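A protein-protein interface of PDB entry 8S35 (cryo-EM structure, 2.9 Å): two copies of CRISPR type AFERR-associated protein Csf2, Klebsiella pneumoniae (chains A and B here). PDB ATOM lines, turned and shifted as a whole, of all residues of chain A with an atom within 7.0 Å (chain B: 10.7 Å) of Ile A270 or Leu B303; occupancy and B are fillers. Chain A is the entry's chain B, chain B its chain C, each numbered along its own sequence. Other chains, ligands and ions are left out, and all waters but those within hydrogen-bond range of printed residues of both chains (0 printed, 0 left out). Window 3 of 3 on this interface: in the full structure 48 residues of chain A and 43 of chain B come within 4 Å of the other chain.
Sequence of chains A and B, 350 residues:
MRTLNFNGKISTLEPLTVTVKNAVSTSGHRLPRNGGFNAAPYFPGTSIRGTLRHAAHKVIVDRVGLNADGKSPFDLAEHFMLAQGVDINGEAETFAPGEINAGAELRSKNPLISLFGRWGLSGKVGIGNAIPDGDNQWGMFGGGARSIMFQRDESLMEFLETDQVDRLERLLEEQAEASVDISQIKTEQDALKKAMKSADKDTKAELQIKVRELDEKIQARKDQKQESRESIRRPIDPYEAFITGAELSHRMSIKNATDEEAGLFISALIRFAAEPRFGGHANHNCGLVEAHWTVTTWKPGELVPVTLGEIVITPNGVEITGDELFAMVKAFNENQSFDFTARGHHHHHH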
ATOM      1  N   ALA A  55     -21.039  12.482   2.109  1.00  0.00           N
ATOM      2  CA  ALA A  55     -21.104  11.393   3.076  1.00  0.00           C
ATOM      3  C   ALA A  55     -19.963  11.491   4.078  1.00  0.00           C
ATOM      4  O   ALA A  55     -20.165  11.350   5.288  1.00  0.00           O
ATOM      5  CB  ALA A  55     -21.071  10.049   2.351  1.00  0.00           C
ATOM      6  N   VAL A  59     -19.905  12.113   8.056  1.00  0.00           N
ATOM      7  CA  VAL A  59     -19.134  11.246   8.944  1.00  0.00           C
ATOM      8  C   VAL A  59     -18.319  12.088   9.913  1.00  0.00           C
ATOM      9  O   VAL A  59     -18.298  11.836  11.122  1.00  0.00           O
ATOM     10  CB  VAL A  59     -18.234  10.300   8.126  1.00  0.00           C
ATOM     11  CG1 VAL A  59     -17.096   9.744   8.983  1.00  0.00           C
ATOM     12  CG2 VAL A  59     -19.055   9.166   7.530  1.00  0.00           C
ATOM     13  N   GLY A 263      -9.032   5.257   6.454  1.00  0.00           N
ATOM     14  CA  GLY A 263     -10.125   4.898   7.339  1.00  0.00           C
ATOM     15  C   GLY A 263     -11.290   5.860   7.232  1.00  0.00           C
ATOM     16  O   GLY A 263     -12.452   5.451   7.275  1.00  0.00           O
ATOM     17  N   LEU A 264     -10.995   7.153   7.099  1.00  0.00           N
ATOM     18  CA  LEU A 264     -12.061   8.126   6.893  1.00  0.00           C
ATOM     19  C   LEU A 264     -12.819   7.832   5.607  1.00  0.00           C
ATOM     20  O   LEU A 264     -14.047   7.931   5.566  1.00  0.00           O
ATOM     21  CB  LEU A 264     -11.490   9.543   6.870  1.00  0.00           C
ATOM     22  CG  LEU A 264     -12.405  10.664   6.366  1.00  0.00           C
ATOM     23  CD1 LEU A 264     -13.781  10.626   7.009  1.00  0.00           C
ATOM     24  CD2 LEU A 264     -11.749  12.007   6.618  1.00  0.00           C
ATOM     25  N   PHE A 265     -12.102   7.468   4.544  1.00  0.00           N
ATOM     26  CA  PHE A 265     -12.775   7.155   3.288  1.00  0.00           C
ATOM     27  C   PHE A 265     -13.655   5.919   3.425  1.00  0.00           C
ATOM     28  O   PHE A 265     -14.773   5.881   2.895  1.00  0.00           O
ATOM     29  CB  PHE A 265     -11.749   6.954   2.177  1.00  0.00           C
ATOM     30  CG  PHE A 265     -12.355   6.854   0.812  1.00  0.00           C
ATOM     31  CD1 PHE A 265     -12.792   7.986   0.152  1.00  0.00           C
ATOM     32  CD2 PHE A 265     -12.493   5.628   0.191  1.00  0.00           C
ATOM     33  CE1 PHE A 265     -13.351   7.897  -1.104  1.00  0.00           C
ATOM     34  CE2 PHE A 265     -13.051   5.534  -1.066  1.00  0.00           C
ATOM     35  CZ  PHE A 265     -13.481   6.670  -1.713  1.00  0.00           C
ATOM     36  N   ILE A 266     -13.169   4.894   4.127  1.00  0.00           N
ATOM     37  CA  ILE A 266     -13.986   3.699   4.318  1.00  0.00           C
ATOM     38  C   ILE A 266     -15.214   4.032   5.153  1.00  0.00           C
ATOM     39  O   ILE A 266     -16.311   3.525   4.896  1.00  0.00           O
ATOM     40  CB  ILE A 266     -13.163   2.559   4.953  1.00  0.00           C
ATOM     41  CG1 ILE A 266     -11.904   2.211   4.134  1.00  0.00           C
ATOM     42  CG2 ILE A 266     -14.035   1.313   5.129  1.00  0.00           C
ATOM     43  CD1 ILE A 266     -11.978   2.454   2.633  1.00  0.00           C
ATOM     44  N   SER A 267     -15.056   4.882   6.170  1.00  0.00           N
ATOM     45  CA  SER A 267     -16.207   5.288   6.964  1.00  0.00           C
ATOM     46  C   SER A 267     -17.190   6.088   6.123  1.00  0.00           C
ATOM     47  O   SER A 267     -18.407   5.985   6.308  1.00  0.00           O
ATOM     48  CB  SER A 267     -15.750   6.101   8.173  1.00  0.00           C
ATOM     49  OG  SER A 267     -15.262   5.254   9.198  1.00  0.00           O
ATOM     50  N   ALA A 268     -16.677   6.889   5.191  1.00  0.00           N
ATOM     51  CA  ALA A 268     -17.549   7.618   4.280  1.00  0.00           C
ATOM     52  C   ALA A 268     -18.347   6.656   3.418  1.00  0.00           C
ATOM     53  O   ALA A 268     -19.547   6.850   3.204  1.00  0.00           O
ATOM     54  CB  ALA A 268     -16.724   8.558   3.408  1.00  0.00           C
ATOM     55  N   LEU A 269     -17.692   5.612   2.910  1.00  0.00           N
ATOM     56  CA  LEU A 269     -18.409   4.595   2.146  1.00  0.00           C
ATOM     57  C   LEU A 269     -19.472   3.922   3.006  1.00  0.00           C
ATOM     58  O   LEU A 269     -20.600   3.691   2.552  1.00  0.00           O
ATOM     59  CB  LEU A 269     -17.431   3.557   1.603  1.00  0.00           C
ATOM     60  CG  LEU A 269     -16.411   4.059   0.584  1.00  0.00           C
ATOM     61  CD1 LEU A 269     -15.323   3.023   0.375  1.00  0.00           C
ATOM     62  CD2 LEU A 269     -17.087   4.394  -0.728  1.00  0.00           C
ATOM     63  N   ILE A 270     -19.125   3.601   4.252  1.00  0.00           N
ATOM     64  CA  ILE A 270     -20.069   2.936   5.144  1.00  0.00           C
ATOM     65  C   ILE A 270     -21.293   3.812   5.363  1.00  0.00           C
ATOM     66  O   ILE A 270     -22.434   3.341   5.311  1.00  0.00           O
ATOM     67  CB  ILE A 270     -19.387   2.585   6.479  1.00  0.00           C
ATOM     68  CG1 ILE A 270     -18.352   1.478   6.277  1.00  0.00           C
ATOM     69  CG2 ILE A 270     -20.422   2.156   7.513  1.00  0.00           C
ATOM     70  CD1 ILE A 270     -17.339   1.384   7.397  1.00  0.00           C
ATOM     71  N   ARG A 271     -21.076   5.103   5.609  1.00  0.00           N
ATOM     72  CA  ARG A 271     -22.209   5.991   5.838  1.00  0.00           C
ATOM     73  C   ARG A 271     -23.014   6.191   4.563  1.00  0.00           C
ATOM     74  O   ARG A 271     -24.246   6.279   4.608  1.00  0.00           O
ATOM     75  CB  ARG A 271     -21.732   7.334   6.381  1.00  0.00           C
ATOM     76  CG  ARG A 271     -22.820   8.077   7.125  1.00  0.00           C
ATOM     77  CD  ARG A 271     -22.672   9.579   7.024  1.00  0.00           C
ATOM     78  NE  ARG A 271     -23.732  10.267   7.749  1.00  0.00           N
ATOM     79  CZ  ARG A 271     -23.818  10.336   9.072  1.00  0.00           C
ATOM     80  NH1 ARG A 271     -22.912   9.777   9.858  1.00  0.00           N
ATOM     81  NH2 ARG A 271     -24.842  10.984   9.622  1.00  0.00           N
ATOM     82  N   PHE A 272     -22.337   6.269   3.417  1.00  0.00           N
ATOM     83  CA  PHE A 272     -23.047   6.374   2.150  1.00  0.00           C
ATOM     84  C   PHE A 272     -23.925   5.157   1.912  1.00  0.00           C
ATOM     85  O   PHE A 272     -24.978   5.263   1.275  1.00  0.00           O
ATOM     86  CB  PHE A 272     -22.043   6.542   1.009  1.00  0.00           C
ATOM     87  CG  PHE A 272     -22.549   6.068  -0.319  1.00  0.00           C
ATOM     88  CD1 PHE A 272     -23.333   6.890  -1.105  1.00  0.00           C
ATOM     89  CD2 PHE A 272     -22.234   4.804  -0.787  1.00  0.00           C
ATOM     90  CE1 PHE A 272     -23.796   6.461  -2.327  1.00  0.00           C
ATOM     91  CE2 PHE A 272     -22.701   4.368  -2.004  1.00  0.00           C
ATOM     92  CZ  PHE A 272     -23.484   5.195  -2.773  1.00  0.00           C
ATOM     93  N   ALA A 273     -23.506   3.994   2.414  1.00  0.00           N
ATOM     94  CA  ALA A 273     -24.308   2.789   2.240  1.00  0.00           C
ATOM     95  C   ALA A 273     -25.679   2.922   2.886  1.00  0.00           C
ATOM     96  O   ALA A 273     -26.622   2.233   2.481  1.00  0.00           O
ATOM     97  CB  ALA A 273     -23.573   1.582   2.813  1.00  0.00           C
ATOM     98  N   ALA A 274     -25.810   3.780   3.901  1.00  0.00           N
ATOM     99  CA  ALA A 274     -27.115   3.992   4.516  1.00  0.00           C
ATOM    100  C   ALA A 274     -28.100   4.581   3.517  1.00  0.00           C
ATOM    101  O   ALA A 274     -29.271   4.185   3.477  1.00  0.00           O
ATOM    102  CB  ALA A 274     -26.978   4.901   5.735  1.00  0.00           C
ATOM    103  N   GLU A 275     -27.641   5.528   2.703  1.00  0.00           N
ATOM    104  CA  GLU A 275     -28.442   6.155   1.652  1.00  0.00           C
ATOM    105  C   GLU A 275     -27.660   6.038   0.351  1.00  0.00           C
ATOM    106  O   GLU A 275     -27.103   7.023  -0.147  1.00  0.00           O
ATOM    107  CB  GLU A 275     -28.756   7.613   1.989  1.00  0.00           C
ATOM    108  CG  GLU A 275     -29.585   8.354   0.940  1.00  0.00           C
ATOM    109  CD  GLU A 275     -30.894   7.659   0.617  1.00  0.00           C
ATOM    110  OE1 GLU A 275     -31.437   6.970   1.504  1.00  0.00           O
ATOM    111  OE2 GLU A 275     -31.377   7.799  -0.526  1.00  0.00           O
ATOM    112  N   ILE A 311     -14.780  -4.137  -0.201  1.00  0.00           N
ATOM    113  CA  ILE A 311     -15.900  -3.395   0.366  1.00  0.00           C
ATOM    114  C   ILE A 311     -17.114  -3.689  -0.499  1.00  0.00           C
ATOM    115  O   ILE A 311     -17.097  -3.423  -1.707  1.00  0.00           O
ATOM    116  CB  ILE A 311     -15.615  -1.885   0.423  1.00  0.00           C
ATOM    117  CG1 ILE A 311     -14.218  -1.626   0.988  1.00  0.00           C
ATOM    118  CG2 ILE A 311     -16.669  -1.172   1.267  1.00  0.00           C
ATOM    119  CD1 ILE A 311     -13.899  -0.166   1.189  1.00  0.00           C
ATOM    120  N   VAL A 312     -18.162  -4.235   0.111  1.00  0.00           N
ATOM    121  CA  VAL A 312     -19.384  -4.604  -0.593  1.00  0.00           C
ATOM    122  C   VAL A 312     -20.545  -3.908   0.096  1.00  0.00           C
ATOM    123  O   VAL A 312     -20.803  -4.146   1.281  1.00  0.00           O
ATOM    124  CB  VAL A 312     -19.590  -6.127  -0.615  1.00  0.00           C
ATOM    125  CG1 VAL A 312     -20.755  -6.495  -1.522  1.00  0.00           C
ATOM    126  CG2 VAL A 312     -18.315  -6.827  -1.064  1.00  0.00           C
ATOM    127  N   ILE A 313     -21.246  -3.058  -0.647  1.00  0.00           N
ATOM    128  CA  ILE A 313     -22.395  -2.314  -0.145  1.00  0.00           C
ATOM    129  C   ILE A 313     -23.635  -2.899  -0.799  1.00  0.00           C
ATOM    130  O   ILE A 313     -23.764  -2.868  -2.028  1.00  0.00           O
ATOM    131  CB  ILE A 313     -22.275  -0.813  -0.445  1.00  0.00           C
ATOM    132  CG1 ILE A 313     -21.101  -0.205   0.326  1.00  0.00           C
ATOM    133  CG2 ILE A 313     -23.574  -0.102  -0.098  1.00  0.00           C
ATOM    134  CD1 ILE A 313     -20.655   1.136  -0.205  1.00  0.00           C
ATOM    135  N   THR A 314     -24.545  -3.423   0.011  1.00  0.00           N
ATOM    136  CA  THR A 314     -25.778  -4.022  -0.467  1.00  0.00           C
ATOM    137  C   THR A 314     -26.908  -3.555   0.432  1.00  0.00           C
ATOM    138  O   THR A 314     -26.666  -3.116   1.561  1.00  0.00           O
ATOM    139  CB  THR A 314     -25.715  -5.556  -0.453  1.00  0.00           C
ATOM    140  OG1 THR A 314     -25.550  -6.015   0.894  1.00  0.00           O
ATOM    141  CG2 THR A 314     -24.558  -6.054  -1.294  1.00  0.00           C
ATOM    142  N   ASN A 316     -28.690  -5.270   2.153  1.00  0.00           N
ATOM    143  CA  ASN A 316     -28.646  -6.101   3.344  1.00  0.00           C
ATOM    144  C   ASN A 316     -27.499  -5.751   4.282  1.00  0.00           C
ATOM    145  O   ASN A 316     -27.464  -6.275   5.400  1.00  0.00           O
ATOM    146  CB  ASN A 316     -28.537  -7.574   2.946  1.00  0.00           C
ATOM    147  CG  ASN A 316     -29.600  -7.986   1.953  1.00  0.00           C
ATOM    148  OD1 ASN A 316     -30.729  -8.298   2.330  1.00  0.00           O
ATOM    149  ND2 ASN A 316     -29.247  -7.984   0.674  1.00  0.00           N
ATOM    150  N   GLY A 317     -26.573  -4.897   3.876  1.00  0.00           N
ATOM    151  CA  GLY A 317     -25.523  -4.463   4.779  1.00  0.00           C
ATOM    152  C   GLY A 317     -24.246  -4.110   4.043  1.00  0.00           C
ATOM    153  O   GLY A 317     -24.166  -4.143   2.817  1.00  0.00           O
ATOM    154  N   VAL A 318     -23.240  -3.766   4.842  1.00  0.00           N
ATOM    155  CA  VAL A 318     -21.905  -3.426   4.368  1.00  0.00           C
ATOM    156  C   VAL A 318     -20.953  -4.507   4.849  1.00  0.00           C
ATOM    157  O   VAL A 318     -20.770  -4.689   6.059  1.00  0.00           O
ATOM    158  CB  VAL A 318     -21.458  -2.045   4.869  1.00  0.00           C
ATOM    159  CG1 VAL A 318     -19.982  -1.825   4.581  1.00  0.00           C
ATOM    160  CG2 VAL A 318     -22.285  -0.965   4.226  1.00  0.00           C
ATOM    161  N   GLU A 319     -20.344  -5.219   3.908  1.00  0.00           N
ATOM    162  CA  GLU A 319     -19.386  -6.274   4.206  1.00  0.00           C
ATOM    163  C   GLU A 319     -17.993  -5.770   3.861  1.00  0.00           C
ATOM    164  O   GLU A 319     -17.713  -5.444   2.702  1.00  0.00           O
ATOM    165  CB  GLU A 319     -19.708  -7.544   3.422  1.00  0.00           C
ATOM    166  CG  GLU A 319     -21.116  -8.067   3.645  1.00  0.00           C
ATOM    167  CD  GLU A 319     -22.125  -7.453   2.695  1.00  0.00           C
ATOM    168  OE1 GLU A 319     -22.178  -6.208   2.607  1.00  0.00           O
ATOM    169  OE2 GLU A 319     -22.865  -8.214   2.037  1.00  0.00           O
ATOM    170  N   ILE A 320     -17.129  -5.707   4.868  1.00  0.00           N
ATOM    171  CA  ILE A 320     -15.741  -5.292   4.711  1.00  0.00           C
ATOM    172  C   ILE A 320     -14.874  -6.492   5.046  1.00  0.00           C
ATOM    173  O   ILE A 320     -14.980  -7.052   6.144  1.00  0.00           O
ATOM    174  CB  ILE A 320     -15.400  -4.091   5.605  1.00  0.00           C
ATOM    175  CG1 ILE A 320     -16.539  -3.071   5.549  1.00  0.00           C
ATOM    176  CG2 ILE A 320     -14.081  -3.464   5.171  1.00  0.00           C
ATOM    177  CD1 ILE A 320     -16.175  -1.696   6.054  1.00  0.00           C
ATOM    178  N   PHE A 326     -10.343  -3.061   8.172  1.00  0.00           N
ATOM    179  CA  PHE A 326     -10.769  -2.881   9.553  1.00  0.00           C
ATOM    180  C   PHE A 326      -9.736  -2.093  10.343  1.00  0.00           C
ATOM    181  O   PHE A 326     -10.090  -1.224  11.148  1.00  0.00           O
ATOM    182  CB  PHE A 326     -11.014  -4.238  10.212  1.00  0.00           C
ATOM    183  CG  PHE A 326     -12.287  -4.906   9.781  1.00  0.00           C
ATOM    184  CD1 PHE A 326     -13.515  -4.307  10.010  1.00  0.00           C
ATOM    185  CD2 PHE A 326     -12.256  -6.138   9.155  1.00  0.00           C
ATOM    186  CE1 PHE A 326     -14.684  -4.924   9.616  1.00  0.00           C
ATOM    187  CE2 PHE A 326     -13.422  -6.759   8.761  1.00  0.00           C
ATOM    188  CZ  PHE A 326     -14.638  -6.151   8.992  1.00  0.00           C
ATOM    189  N   VAL A 329     -10.013   1.582   9.380  1.00  0.00           N
ATOM    190  CA  VAL A 329     -11.209   2.201   9.943  1.00  0.00           C
ATOM    191  C   VAL A 329     -11.017   2.448  11.433  1.00  0.00           C
ATOM    192  O   VAL A 329     -11.347   3.525  11.948  1.00  0.00           O
ATOM    193  CB  VAL A 329     -12.444   1.324   9.667  1.00  0.00           C
ATOM    194  CG1 VAL A 329     -13.647   1.820  10.464  1.00  0.00           C
ATOM    195  CG2 VAL A 329     -12.752   1.297   8.177  1.00  0.00           C
ATOM    196  N   THR B 297     -34.615   0.036   8.198  1.00  0.00           N
ATOM    197  CA  THR B 297     -33.957   1.288   8.529  1.00  0.00           C
ATOM    198  C   THR B 297     -32.453   1.074   8.549  1.00  0.00           C
ATOM    199  O   THR B 297     -31.962  -0.049   8.680  1.00  0.00           O
ATOM    200  CB  THR B 297     -34.435   1.834   9.881  1.00  0.00           C
ATOM    201  OG1 THR B 297     -33.825   3.107  10.121  1.00  0.00           O
ATOM    202  CG2 THR B 297     -34.090   0.885  11.032  1.00  0.00           C
ATOM    203  N   TRP B 298     -31.719   2.173   8.405  1.00  0.00           N
ATOM    204  CA  TRP B 298     -30.262   2.107   8.373  1.00  0.00           C
ATOM    205  C   TRP B 298     -29.733   3.385   9.014  1.00  0.00           C
ATOM    206  O   TRP B 298     -29.645   4.424   8.355  1.00  0.00           O
ATOM    207  CB  TRP B 298     -29.757   1.941   6.946  1.00  0.00           C
ATOM    208  CG  TRP B 298     -28.411   1.307   6.853  1.00  0.00           C
ATOM    209  CD1 TRP B 298     -27.385   1.420   7.744  1.00  0.00           C
ATOM    210  CD2 TRP B 298     -27.939   0.461   5.802  1.00  0.00           C
ATOM    211  NE1 TRP B 298     -26.304   0.693   7.313  1.00  0.00           N
ATOM    212  CE2 TRP B 298     -26.619   0.095   6.123  1.00  0.00           C
ATOM    213  CE3 TRP B 298     -28.505  -0.024   4.621  1.00  0.00           C
ATOM    214  CZ2 TRP B 298     -25.857  -0.733   5.307  1.00  0.00           C
ATOM    215  CZ3 TRP B 298     -27.747  -0.845   3.812  1.00  0.00           C
ATOM    216  CH2 TRP B 298     -26.438  -1.190   4.157  1.00  0.00           C
ATOM    217  N   LYS B 299     -29.396   3.301  10.291  1.00  0.00           N
ATOM    218  CA  LYS B 299     -28.783   4.434  10.960  1.00  0.00           C
ATOM    219  C   LYS B 299     -27.444   4.723  10.287  1.00  0.00           C
ATOM    220  O   LYS B 299     -26.622   3.807  10.155  1.00  0.00           O
ATOM    221  CB  LYS B 299     -28.578   4.147  12.444  1.00  0.00           C
ATOM    222  CG  LYS B 299     -28.138   5.363  13.242  1.00  0.00           C
ATOM    223  CD  LYS B 299     -28.069   5.070  14.733  1.00  0.00           C
ATOM    224  CE  LYS B 299     -26.811   4.298  15.105  1.00  0.00           C
ATOM    225  NZ  LYS B 299     -25.565   5.085  14.884  1.00  0.00           N
ATOM    226  N   PRO B 300     -27.196   5.950   9.817  1.00  0.00           N
ATOM    227  CA  PRO B 300     -25.917   6.220   9.150  1.00  0.00           C
ATOM    228  C   PRO B 300     -24.739   5.888  10.053  1.00  0.00           C
ATOM    229  O   PRO B 300     -24.741   6.191  11.248  1.00  0.00           O
ATOM    230  CB  PRO B 300     -25.988   7.719   8.843  1.00  0.00           C
ATOM    231  CG  PRO B 300     -27.423   8.016   8.755  1.00  0.00           C
ATOM    232  CD  PRO B 300     -28.092   7.119   9.747  1.00  0.00           C
ATOM    233  N   GLY B 301     -23.732   5.250   9.464  1.00  0.00           N
ATOM    234  CA  GLY B 301     -22.588   4.750  10.187  1.00  0.00           C
ATOM    235  C   GLY B 301     -22.692   3.293  10.588  1.00  0.00           C
ATOM    236  O   GLY B 301     -21.665   2.674  10.885  1.00  0.00           O
ATOM    237  N   GLU B 302     -23.897   2.731  10.605  1.00  0.00           N
ATOM    238  CA  GLU B 302     -24.065   1.321  10.917  1.00  0.00           C
ATOM    239  C   GLU B 302     -23.728   0.467   9.704  1.00  0.00           C
ATOM    240  O   GLU B 302     -23.888   0.888   8.556  1.00  0.00           O
ATOM    241  CB  GLU B 302     -25.497   1.034  11.366  1.00  0.00           C
ATOM    242  CG  GLU B 302     -25.834   1.564  12.747  1.00  0.00           C
ATOM    243  CD  GLU B 302     -25.111   0.821  13.852  1.00  0.00           C
ATOM    244  OE1 GLU B 302     -24.466  -0.207  13.560  1.00  0.00           O
ATOM    245  OE2 GLU B 302     -25.190   1.267  15.016  1.00  0.00           O
ATOM    246  N   LEU B 303     -23.260  -0.751   9.971  1.00  0.00           N
ATOM    247  CA  LEU B 303     -22.856  -1.657   8.906  1.00  0.00           C
ATOM    248  C   LEU B 303     -23.991  -2.527   8.389  1.00  0.00           C
ATOM    249  O   LEU B 303     -23.859  -3.096   7.298  1.00  0.00           O
ATOM    250  CB  LEU B 303     -21.724  -2.566   9.393  1.00  0.00           C
ATOM    251  CG  LEU B 303     -20.431  -1.863   9.804  1.00  0.00           C
ATOM    252  CD1 LEU B 303     -19.583  -2.773  10.675  1.00  0.00           C
ATOM    253  CD2 LEU B 303     -19.655  -1.418   8.580  1.00  0.00           C
ATOM    254  N   VAL B 304     -25.087  -2.650   9.135  1.00  0.00           N
ATOM    255  CA  VAL B 304     -26.217  -3.482   8.714  1.00  0.00           C
ATOM    256  C   VAL B 304     -27.513  -2.729   8.953  1.00  0.00           C
ATOM    257  O   VAL B 304     -27.603  -1.865   9.836  1.00  0.00           O
ATOM    258  CB  VAL B 304     -26.256  -4.825   9.471  1.00  0.00           C
ATOM    259  CG1 VAL B 304     -24.975  -5.605   9.227  1.00  0.00           C
ATOM    260  CG2 VAL B 304     -26.479  -4.603  10.965  1.00  0.00           C
ATOM    261  N   PRO B 305     -28.547  -3.040   8.174  1.00  0.00           N
ATOM    262  CA  PRO B 305     -29.863  -2.453   8.425  1.00  0.00           C
ATOM    263  C   PRO B 305     -30.610  -3.225   9.505  1.00  0.00           C
ATOM    264  O   PRO B 305     -30.214  -4.314   9.918  1.00  0.00           O
ATOM    265  CB  PRO B 305     -30.560  -2.579   7.072  1.00  0.00           C
ATOM    266  CG  PRO B 305     -30.019  -3.840   6.522  1.00  0.00           C
ATOM    267  CD  PRO B 305     -28.594  -3.956   7.018  1.00  0.00           C
ATOM    268  N   VAL B 306     -31.712  -2.633   9.955  1.00  0.00           N
ATOM    269  CA  VAL B 306     -32.605  -3.244  10.932  1.00  0.00           C
ATOM    270  C   VAL B 306     -33.992  -3.305  10.314  1.00  0.00           C
ATOM    271  O   VAL B 306     -34.530  -2.278   9.887  1.00  0.00           O
ATOM    272  CB  VAL B 306     -32.627  -2.457  12.255  1.00  0.00           C
ATOM    273  CG1 VAL B 306     -33.588  -3.105  13.251  1.00  0.00           C
ATOM    274  CG2 VAL B 306     -31.218  -2.357  12.834  1.00  0.00           C
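Hydrophobic or aromatic side chains of chain B within 4 Å of the printed part of chain A: Trp B298, Pro B300, Leu B303 and Pro B305. Of the 26 printed residues of chain A, 8 touch a printed residue of chain B. Printed residues of chain A that touch a printed residue of chain B: Ile A270, Arg A271, Ala A273, Ala A274, Thr A314, Asn A316, Gly A317 and Val A318. Hydrophobic or aromatic side chains of chain A within 4 Å of the printed part of chain B: Ile A270, Ala A274 and Val A318. Among the printed residues, no Asp or Glu carboxylate lies within 4 Å of a Lys or Arg side-chain nitrogen of the other chain.
N of Val A318 lies within hydrogen-bond range of O of Leu B303.
N of Asn A316 sits close to OG1 of Thr A314. The side-chain hydroxyl (OG1) of Thr A314 lies within hydrogen-bond range of the backbone carbonyl oxygen (O) of Gly A317, at 3.0 Å. The backbone carbonyl oxygen (O) of Glu B302 lies within hydrogen-bond range of the indole nitrogen (NE1) of Trp B298. OE2 of Glu B302 lies within salt-bridge range of NZ of Lys B299 (3.8 Å).
No residue of chain B comes within 4 Å of Ser A267. No residue of chain B comes within 4 Å of Ala A268. No residue of chain B comes within 4 Å of Leu A269. Of chain B, only Gly B301, Glu B302 and Leu B303 come within 4 Å of Ile A270. Of chain B, only Trp B298 comes within 4 Å of Ala A273. Of the printed residues of chain B, Gly A317 touches Trp B298, Leu B303 and Pro B305. Of chain B, only Trp B298 (3.7 Å) and Leu B303 (2.6 Å) come within 4 Å of Val A318. Printed residues of chain A within 4 Å of Pro B300: Arg A271 (3.4 Å) and Ala A274 (3.8 Å). Printed residues of chain A within 4 Å of Gly B301: Ile A270 and Arg A271. Of the printed residues of chain A, Glu B302 touches Ile A270 (3.8 Å). Leu B303 touches three residues of chain A. The nearest residue of chain B that does not touch Ile A270 is Trp B298 (5.1 Å).
Gly B301 touches Ile A270 (O to CG2, 3.6 Å). Ile A270 touches Glu B302 (CG2 to O, 3.8 Å). CG2 of Ile A270 touches CD2 of Leu B303, at 3.8 Å. Pro B300 touches Arg A271. Arg A271 touches Gly B301. CZ3 of Trp B298 touches O of Ala A273, at 3.5 Å. CA of Pro B300 touches CB of Ala A274, 3.8 Å away. Gly A317 touches Trp B298 (CA to CH2, 3.5 Å). CA of Gly A317 touches CD of Pro B305, at 3.8 Å. Val A318 touches Trp B298.
No position is printed for both chains.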
